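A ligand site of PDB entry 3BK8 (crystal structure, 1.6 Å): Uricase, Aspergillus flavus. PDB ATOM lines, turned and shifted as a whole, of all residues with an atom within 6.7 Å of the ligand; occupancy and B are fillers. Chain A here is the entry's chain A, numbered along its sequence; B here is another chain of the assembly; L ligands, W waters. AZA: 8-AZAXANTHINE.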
ATOM      1  N   SER A 157      29.440 -11.148 -12.723  1.00  0.00           N
ATOM      2  CA  SER A 157      28.486 -10.493 -11.839  1.00  0.00           C
ATOM      3  C   SER A 157      27.312 -11.447 -11.612  1.00  0.00           C
ATOM      4  O   SER A 157      26.798 -12.063 -12.558  1.00  0.00           O
ATOM      5  CB  SER A 157      28.027  -9.133 -12.374  1.00  0.00           C
ATOM      6  OG  SER A 157      26.990  -8.541 -11.595  1.00  0.00           O
ATOM      7  N   GLN A 158      26.907 -11.540 -10.345  1.00  0.00           N
ATOM      8  CA  GLN A 158      25.798 -12.349  -9.881  1.00  0.00           C
ATOM      9  C   GLN A 158      24.826 -11.551  -9.038  1.00  0.00           C
ATOM     10  O   GLN A 158      25.161 -10.520  -8.455  1.00  0.00           O
ATOM     11  CB  GLN A 158      26.346 -13.541  -9.073  1.00  0.00           C
ATOM     12  CG  GLN A 158      27.407 -14.335  -9.791  1.00  0.00           C
ATOM     13  CD  GLN A 158      27.792 -15.616  -9.073  1.00  0.00           C
ATOM     14  OE1 GLN A 158      27.018 -16.098  -8.232  1.00  0.00           O
ATOM     15  NE2 GLN A 158      28.980 -16.121  -9.370  1.00  0.00           N
ATOM     16  N   PHE A 159      23.581 -12.036  -8.940  1.00  0.00           N
ATOM     17  CA  PHE A 159      22.663 -11.452  -7.978  1.00  0.00           C
ATOM     18  C   PHE A 159      21.598 -12.491  -7.636  1.00  0.00           C
ATOM     19  O   PHE A 159      20.655 -12.690  -8.400  1.00  0.00           O
ATOM     20  CB  PHE A 159      22.053 -10.149  -8.493  1.00  0.00           C
ATOM     21  CG  PHE A 159      21.297  -9.418  -7.382  1.00  0.00           C
ATOM     22  CD1 PHE A 159      22.052  -9.008  -6.278  1.00  0.00           C
ATOM     23  CD2 PHE A 159      19.936  -9.173  -7.403  1.00  0.00           C
ATOM     24  CE1 PHE A 159      21.371  -8.363  -5.251  1.00  0.00           C
ATOM     25  CE2 PHE A 159      19.258  -8.520  -6.396  1.00  0.00           C
ATOM     26  CZ  PHE A 159      20.026  -8.106  -5.303  1.00  0.00           C
ATOM     27  N   PHE A 162      18.380 -12.628  -2.755  1.00  0.00           N
ATOM     28  CA  PHE A 162      17.621 -11.481  -2.288  1.00  0.00           C
ATOM     29  C   PHE A 162      16.210 -11.867  -1.840  1.00  0.00           C
ATOM     30  O   PHE A 162      15.723 -12.957  -2.183  1.00  0.00           O
ATOM     31  CB  PHE A 162      17.504 -10.384  -3.361  1.00  0.00           C
ATOM     32  CG  PHE A 162      17.025 -10.888  -4.711  1.00  0.00           C
ATOM     33  CD1 PHE A 162      17.935 -11.431  -5.593  1.00  0.00           C
ATOM     34  CD2 PHE A 162      15.673 -10.794  -5.012  1.00  0.00           C
ATOM     35  CE1 PHE A 162      17.512 -11.903  -6.836  1.00  0.00           C
ATOM     36  CE2 PHE A 162      15.254 -11.256  -6.256  1.00  0.00           C
ATOM     37  CZ  PHE A 162      16.174 -11.781  -7.118  1.00  0.00           C
ATOM     38  N   LEU A 170      11.775 -10.485 -10.172  1.00  0.00           N
ATOM     39  CA  LEU A 170      13.136 -10.724 -10.602  1.00  0.00           C
ATOM     40  C   LEU A 170      13.620 -12.153 -10.389  1.00  0.00           C
ATOM     41  O   LEU A 170      13.511 -12.684  -9.266  1.00  0.00           O
ATOM     42  CB  LEU A 170      14.073  -9.769  -9.844  1.00  0.00           C
ATOM     43  CG  LEU A 170      15.529  -9.799 -10.281  1.00  0.00           C
ATOM     44  CD1 LEU A 170      15.617  -9.382 -11.732  1.00  0.00           C
ATOM     45  CD2 LEU A 170      16.357  -8.873  -9.396  1.00  0.00           C
ATOM     46  N   ARG A 176      25.436 -12.228 -15.090  1.00  0.00           N
ATOM     47  CA  ARG A 176      24.740 -11.087 -15.659  1.00  0.00           C
ATOM     48  C   ARG A 176      25.789 -10.030 -16.050  1.00  0.00           C
ATOM     49  O   ARG A 176      26.940 -10.153 -15.647  1.00  0.00           O
ATOM     50  CB  ARG A 176      23.726 -10.422 -14.742  1.00  0.00           C
ATOM     51  CG  ARG A 176      24.335  -9.853 -13.470  1.00  0.00           C
ATOM     52  CD  ARG A 176      23.358  -9.206 -12.525  1.00  0.00           C
ATOM     53  NE  ARG A 176      24.070  -8.461 -11.452  1.00  0.00           N
ATOM     54  CZ  ARG A 176      23.442  -7.670 -10.609  1.00  0.00           C
ATOM     55  NH1 ARG A 176      22.138  -7.489 -10.633  1.00  0.00           N
ATOM     56  NH2 ARG A 176      24.189  -7.038  -9.667  1.00  0.00           N
ATOM     57  N   LEU A 178      27.180  -6.264 -15.611  1.00  0.00           N
ATOM     58  CA  LEU A 178      27.118  -5.173 -14.644  1.00  0.00           C
ATOM     59  C   LEU A 178      27.790  -3.945 -15.285  1.00  0.00           C
ATOM     60  O   LEU A 178      28.927  -4.004 -15.733  1.00  0.00           O
ATOM     61  CB  LEU A 178      27.806  -5.553 -13.340  1.00  0.00           C
ATOM     62  CG  LEU A 178      27.907  -4.462 -12.263  1.00  0.00           C
ATOM     63  CD1 LEU A 178      26.550  -3.977 -11.795  1.00  0.00           C
ATOM     64  CD2 LEU A 178      28.686  -5.005 -11.063  1.00  0.00           C
ATOM     65  N   SER A 224      31.395 -10.437  -8.577  1.00  0.00           N
ATOM     66  CA  SER A 224      30.493  -9.653  -7.758  1.00  0.00           C
ATOM     67  C   SER A 224      29.229 -10.327  -7.287  1.00  0.00           C
ATOM     68  O   SER A 224      28.445 -10.846  -8.097  1.00  0.00           O
ATOM     69  CB  SER A 224      30.069  -8.413  -8.594  1.00  0.00           C
ATOM     70  OG  SER A 224      29.103  -7.701  -7.851  1.00  0.00           O
ATOM     71  N   ALA A 225      28.966 -10.300  -5.979  1.00  0.00           N
ATOM     72  CA  ALA A 225      27.747 -10.813  -5.391  1.00  0.00           C
ATOM     73  C   ALA A 225      26.574  -9.846  -5.449  1.00  0.00           C
ATOM     74  O   ALA A 225      25.400 -10.219  -5.316  1.00  0.00           O
ATOM     75  CB  ALA A 225      28.001 -11.178  -3.921  1.00  0.00           C
ATOM     76  N   SER A 226      26.886  -8.576  -5.668  1.00  0.00           N
ATOM     77  CA  SER A 226      25.966  -7.468  -5.722  1.00  0.00           C
ATOM     78  C   SER A 226      26.786  -6.175  -5.911  1.00  0.00           C
ATOM     79  O   SER A 226      28.004  -6.148  -5.703  1.00  0.00           O
ATOM     80  CB  SER A 226      25.077  -7.316  -4.488  1.00  0.00           C
ATOM     81  OG  SER A 226      25.896  -6.960  -3.367  1.00  0.00           O
ATOM     82  N   VAL A 227      26.091  -5.117  -6.309  1.00  0.00           N
ATOM     83  CA  VAL A 227      26.785  -3.822  -6.370  1.00  0.00           C
ATOM     84  C   VAL A 227      27.217  -3.416  -4.967  1.00  0.00           C
ATOM     85  O   VAL A 227      28.343  -2.972  -4.787  1.00  0.00           O
ATOM     86  CB  VAL A 227      25.844  -2.781  -6.993  1.00  0.00           C
ATOM     87  CG1 VAL A 227      26.491  -1.413  -6.943  1.00  0.00           C
ATOM     88  CG2 VAL A 227      25.503  -3.179  -8.433  1.00  0.00           C
ATOM     89  N   GLN A 228      26.336  -3.660  -4.011  1.00  0.00           N
ATOM     90  CA  GLN A 228      26.615  -3.377  -2.597  1.00  0.00           C
ATOM     91  C   GLN A 228      27.917  -4.025  -2.148  1.00  0.00           C
ATOM     92  O   GLN A 228      28.823  -3.419  -1.556  1.00  0.00           O
ATOM     93  CB  GLN A 228      25.466  -3.870  -1.723  1.00  0.00           C
ATOM     94  CG  GLN A 228      24.145  -3.121  -1.830  1.00  0.00           C
ATOM     95  CD  GLN A 228      23.202  -3.592  -2.923  1.00  0.00           C
ATOM     96  OE1 GLN A 228      23.607  -4.163  -3.934  1.00  0.00           O
ATOM     97  NE2 GLN A 228      21.921  -3.324  -2.738  1.00  0.00           N
ATOM     98  N   ASN A 254      22.908   0.962 -11.125  1.00  0.00           N
ATOM     99  CA  ASN A 254      22.966  -0.319 -11.840  1.00  0.00           C
ATOM    100  C   ASN A 254      22.282  -0.078 -13.194  1.00  0.00           C
ATOM    101  O   ASN A 254      21.070   0.021 -13.253  1.00  0.00           O
ATOM    102  CB  ASN A 254      22.283  -1.352 -10.950  1.00  0.00           C
ATOM    103  CG  ASN A 254      22.506  -2.784 -11.353  1.00  0.00           C
ATOM    104  OD1 ASN A 254      23.189  -3.013 -12.343  1.00  0.00           O
ATOM    105  ND2 ASN A 254      21.951  -3.730 -10.591  1.00  0.00           N
ATOM    106  N   HIS A 256      20.982  -1.312 -16.112  1.00  0.00           N
ATOM    107  CA  HIS A 256      20.602  -2.672 -16.490  1.00  0.00           C
ATOM    108  C   HIS A 256      20.680  -2.949 -17.995  1.00  0.00           C
ATOM    109  O   HIS A 256      20.357  -2.085 -18.814  1.00  0.00           O
ATOM    110  CB  HIS A 256      19.186  -2.941 -16.002  1.00  0.00           C
ATOM    111  CG  HIS A 256      18.929  -2.587 -14.567  1.00  0.00           C
ATOM    112  ND1 HIS A 256      19.460  -3.312 -13.511  1.00  0.00           N
ATOM    113  CD2 HIS A 256      18.224  -1.588 -14.002  1.00  0.00           C
ATOM    114  CE1 HIS A 256      19.058  -2.771 -12.379  1.00  0.00           C
ATOM    115  NE2 HIS A 256      18.313  -1.716 -12.634  1.00  0.00           N
ATOM    116  N   GLY A 286      18.579   0.801 -10.816  1.00  0.00           N
ATOM    117  CA  GLY A 286      18.892   0.708  -9.391  1.00  0.00           C
ATOM    118  C   GLY A 286      19.917   1.793  -9.050  1.00  0.00           C
ATOM    119  O   GLY A 286      20.704   2.235  -9.882  1.00  0.00           O
ATOM    120  N   ILE A 288      22.645   2.511  -5.852  1.00  0.00           N
ATOM    121  CA  ILE A 288      23.203   1.846  -4.658  1.00  0.00           C
ATOM    122  C   ILE A 288      24.218   2.790  -4.015  1.00  0.00           C
ATOM    123  O   ILE A 288      25.077   3.255  -4.771  1.00  0.00           O
ATOM    124  CB  ILE A 288      23.868   0.504  -5.008  1.00  0.00           C
ATOM    125  CG1 ILE A 288      23.088  -0.361  -6.017  1.00  0.00           C
ATOM    126  CG2 ILE A 288      24.140  -0.270  -3.716  1.00  0.00           C
ATOM    127  CD1 ILE A 288      21.635  -0.551  -5.708  1.00  0.00           C
ATOM    128  N   TYR B   8      19.695   2.369  -0.746  1.00  0.00           N
ATOM    129  CA  TYR B   8      19.730   1.817  -2.107  1.00  0.00           C
ATOM    130  C   TYR B   8      18.270   1.781  -2.540  1.00  0.00           C
ATOM    131  O   TYR B   8      17.331   1.729  -1.753  1.00  0.00           O
ATOM    132  CB  TYR B   8      20.414   0.433  -2.137  1.00  0.00           C
ATOM    133  CG  TYR B   8      19.356  -0.597  -1.775  1.00  0.00           C
ATOM    134  CD1 TYR B   8      18.923  -0.663  -0.446  1.00  0.00           C
ATOM    135  CD2 TYR B   8      18.759  -1.440  -2.705  1.00  0.00           C
ATOM    136  CE1 TYR B   8      17.959  -1.559  -0.031  1.00  0.00           C
ATOM    137  CE2 TYR B   8      17.780  -2.319  -2.309  1.00  0.00           C
ATOM    138  CZ  TYR B   8      17.388  -2.371  -0.993  1.00  0.00           C
ATOM    139  OH  TYR B   8      16.406  -3.272  -0.637  1.00  0.00           O
ATOM    140  N   GLY B   9      18.105   1.736  -3.873  1.00  0.00           N
ATOM    141  CA  GLY B   9      16.736   1.551  -4.340  1.00  0.00           C
ATOM    142  C   GLY B   9      16.674   1.705  -5.851  1.00  0.00           C
ATOM    143  O   GLY B   9      17.630   1.382  -6.526  1.00  0.00           O
ATOM    144  N   LYS B  10      15.508   2.172  -6.256  1.00  0.00           N
ATOM    145  CA  LYS B  10      15.284   2.332  -7.696  1.00  0.00           C
ATOM    146  C   LYS B  10      15.051   3.798  -8.014  1.00  0.00           C
ATOM    147  O   LYS B  10      14.208   4.433  -7.368  1.00  0.00           O
ATOM    148  CB  LYS B  10      14.110   1.475  -8.171  1.00  0.00           C
ATOM    149  CG  LYS B  10      14.059   1.387  -9.690  1.00  0.00           C
ATOM    150  CD  LYS B  10      15.137   0.523 -10.268  1.00  0.00           C
ATOM    151  CE  LYS B  10      14.663  -0.859 -10.710  1.00  0.00           C
ATOM    152  NZ  LYS B  10      15.814  -1.761 -11.032  1.00  0.00           N
ATOM    153  N   ASN B  51      22.580 -11.035   0.649  1.00  0.00           N
ATOM    154  CA  ASN B  51      21.495 -10.374  -0.073  1.00  0.00           C
ATOM    155  C   ASN B  51      20.141 -10.647   0.551  1.00  0.00           C
ATOM    156  O   ASN B  51      19.109 -10.092   0.147  1.00  0.00           O
ATOM    157  CB  ASN B  51      21.502 -10.793  -1.543  1.00  0.00           C
ATOM    158  CG  ASN B  51      22.725 -10.300  -2.291  1.00  0.00           C
ATOM    159  OD1 ASN B  51      23.246  -9.229  -2.000  1.00  0.00           O
ATOM    160  ND2 ASN B  51      23.221 -11.051  -3.266  1.00  0.00           N
ATOM    161  N   ILE B  54      18.091  -7.623   1.180  1.00  0.00           N
ATOM    162  CA  ILE B  54      17.783  -6.722   0.070  1.00  0.00           C
ATOM    163  C   ILE B  54      16.421  -7.006  -0.558  1.00  0.00           C
ATOM    164  O   ILE B  54      16.172  -8.121  -1.035  1.00  0.00           O
ATOM    165  CB  ILE B  54      18.855  -6.749  -1.026  1.00  0.00           C
ATOM    166  CG1 ILE B  54      20.264  -6.307  -0.612  1.00  0.00           C
ATOM    167  CG2 ILE B  54      18.393  -5.897  -2.217  1.00  0.00           C
ATOM    168  CD1 ILE B  54      20.320  -4.898  -0.036  1.00  0.00           C
ATOM    169  N   VAL B  55      15.603  -5.970  -0.528  1.00  0.00           N
ATOM    170  CA  VAL B  55      14.362  -5.916  -1.295  1.00  0.00           C
ATOM    171  C   VAL B  55      14.847  -5.521  -2.690  1.00  0.00           C
ATOM    172  O   VAL B  55      15.229  -4.349  -2.782  1.00  0.00           O
ATOM    173  CB  VAL B  55      13.349  -4.928  -0.712  1.00  0.00           C
ATOM    174  CG1 VAL B  55      12.150  -4.710  -1.614  1.00  0.00           C
ATOM    175  CG2 VAL B  55      12.917  -5.395   0.690  1.00  0.00           C
ATOM    176  N   ALA B  56      14.874  -6.415  -3.676  1.00  0.00           N
ATOM    177  CA  ALA B  56      15.491  -6.060  -4.958  1.00  0.00           C
ATOM    178  C   ALA B  56      14.918  -4.767  -5.525  1.00  0.00           C
ATOM    179  O   ALA B  56      13.732  -4.491  -5.316  1.00  0.00           O
ATOM    180  CB  ALA B  56      15.245  -7.175  -5.987  1.00  0.00           C
ATOM    181  N   THR B  57      15.777  -3.984  -6.204  1.00  0.00           N
ATOM    182  CA  THR B  57      15.303  -2.719  -6.756  1.00  0.00           C
ATOM    183  C   THR B  57      14.216  -2.968  -7.812  1.00  0.00           C
ATOM    184  O   THR B  57      13.289  -2.174  -7.933  1.00  0.00           O
ATOM    185  CB  THR B  57      16.455  -1.879  -7.332  1.00  0.00           C
ATOM    186  OG1 THR B  57      17.082  -2.533  -8.437  1.00  0.00           O
ATOM    187  CG2 THR B  57      17.555  -1.692  -6.267  1.00  0.00           C
ATOM    188  N   ASP B  58      14.319  -4.124  -8.470  1.00  0.00           N
ATOM    189  CA  ASP B  58      13.239  -4.485  -9.384  1.00  0.00           C
ATOM    190  C   ASP B  58      11.906  -4.664  -8.642  1.00  0.00           C
ATOM    191  O   ASP B  58      10.863  -4.274  -9.154  1.00  0.00           O
ATOM    192  CB  ASP B  58      13.645  -5.765 -10.130  1.00  0.00           C
ATOM    193  CG  ASP B  58      12.625  -6.194 -11.168  1.00  0.00           C
ATOM    194  OD1 ASP B  58      12.720  -5.726 -12.339  1.00  0.00           O
ATOM    195  OD2 ASP B  58      11.722  -7.002 -10.847  1.00  0.00           O
ATOM    196  N   SER B  59      11.952  -5.235  -7.408  1.00  0.00           N
ATOM    197  CA  SER B  59      10.701  -5.321  -6.662  1.00  0.00           C
ATOM    198  C   SER B  59      10.186  -3.984  -6.191  1.00  0.00           C
ATOM    199  O   SER B  59       9.002  -3.691  -6.112  1.00  0.00           O
ATOM    200  CB  SER B  59      10.884  -6.301  -5.473  1.00  0.00           C
ATOM    201  OG  SER B  59      11.555  -7.438  -5.995  1.00  0.00           O
HETATM  202  N1  AZA L   1      21.749  -4.925  -6.061  1.00  0.00           N
HETATM  203  C2  AZA L   1      22.303  -5.476  -7.192  1.00  0.00           C
HETATM  204  O2  AZA L   1      23.494  -5.617  -7.342  1.00  0.00           O
HETATM  205  N3  AZA L   1      21.452  -5.888  -8.180  1.00  0.00           N
HETATM  206  C4  AZA L   1      20.122  -5.696  -7.972  1.00  0.00           C
HETATM  207  C5  AZA L   1      19.560  -5.162  -6.821  1.00  0.00           C
HETATM  208  C6  AZA L   1      20.425  -4.732  -5.754  1.00  0.00           C
HETATM  209  O6  AZA L   1      20.035  -4.179  -4.713  1.00  0.00           O
HETATM  210  N7  AZA L   1      18.248  -5.169  -6.873  1.00  0.00           N
HETATM  211  N8  AZA L   1      17.970  -5.669  -8.074  1.00  0.00           N
HETATM  212  N9  AZA L   1      19.080  -6.038  -8.799  1.00  0.00           N
HETATM  213  O   HOH W   1      19.145  -6.619 -11.383  1.00  0.00           O
HETATM  214  O   HOH W   2      19.789  -2.577  -8.718  1.00  0.00           O
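The guanidinium group (NH2) of Arg 176 lies within hydrogen-bond range of an oxygen (O2) of the ligand, at 2.8 Å.
N7 of the ligand is in hydrogen-bond range of N of Thr 57 of chain B (2.8 Å).
A nitrogen (N8) of the ligand sits at hydrogen-bond distance from the side-chain hydroxyl (OG1) of Thr 57 of chain B (3.3 Å).
An oxygen (O2) of the ligand sits at hydrogen-bond distance from the backbone NH of Val 227 (2.8 Å).
The side-chain amide nitrogen of Gln 228 sits at hydrogen-bond distance from an oxygen (O6) of the ligand (2.9 Å).
The side-chain amide nitrogen of Asn 254 sits close to a nitrogen (N3) of the ligand (3.3 Å).
The backbone NH (N) of Arg 176 sits at hydrogen-bond distance from the backbone carbonyl oxygen (O) of Ser 157.
The side-chain hydroxyl (OG1) of Thr 57 of chain B is in hydrogen-bond range of the side-chain amino group (NZ) of Lys 10 of chain B, 3.0 Å away.
The backbone NH (N) of Gln 228 sits close to the side-chain hydroxyl (OG) of Ser 226.
O of Asn 254 lies within hydrogen-bond range of NE2 of His 256 (3.3 Å).
N of Asn 254 is in hydrogen-bond range of O of Gly 286, at 2.8 Å.
The side-chain hydroxyl of Ser 224 sits at hydrogen-bond distance from the backbone carbonyl oxygen of Ser 226.
The backbone carbonyl oxygen of Val 55 of chain B is in hydrogen-bond range of the side-chain hydroxyl of Tyr 8 of chain B (2.7 Å).
Merely in contact with the ligand: Phe 159 (3.3 Å), Leu 170 (3.8 Å), Ser 226 (3.5 Å), Tyr 8 of chain B (3.6 Å), Ile 54 of chain B (3.4 Å), Ala 56 of chain B (3.5 Å) and Asp 58 of chain B (3.98 Å).
Hydrophobic or aromatic side chains within 4 Å of the ligand: Phe 159, Leu 170, Val 227, Tyr 8 of chain B, Ile 54 of chain B and Ala 56 of chain B.
Water W1 lies within hydrogen-bond range of N9 of the ligand (2.6 Å) and NH1 of Arg 176 (3.2 Å).
Water W2 lies within hydrogen-bond range of the side-chain hydroxyl (OG1) of Thr 57 of chain B (2.7 Å) and the side-chain amide nitrogen (ND2) of Asn 254 (3.1 Å).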
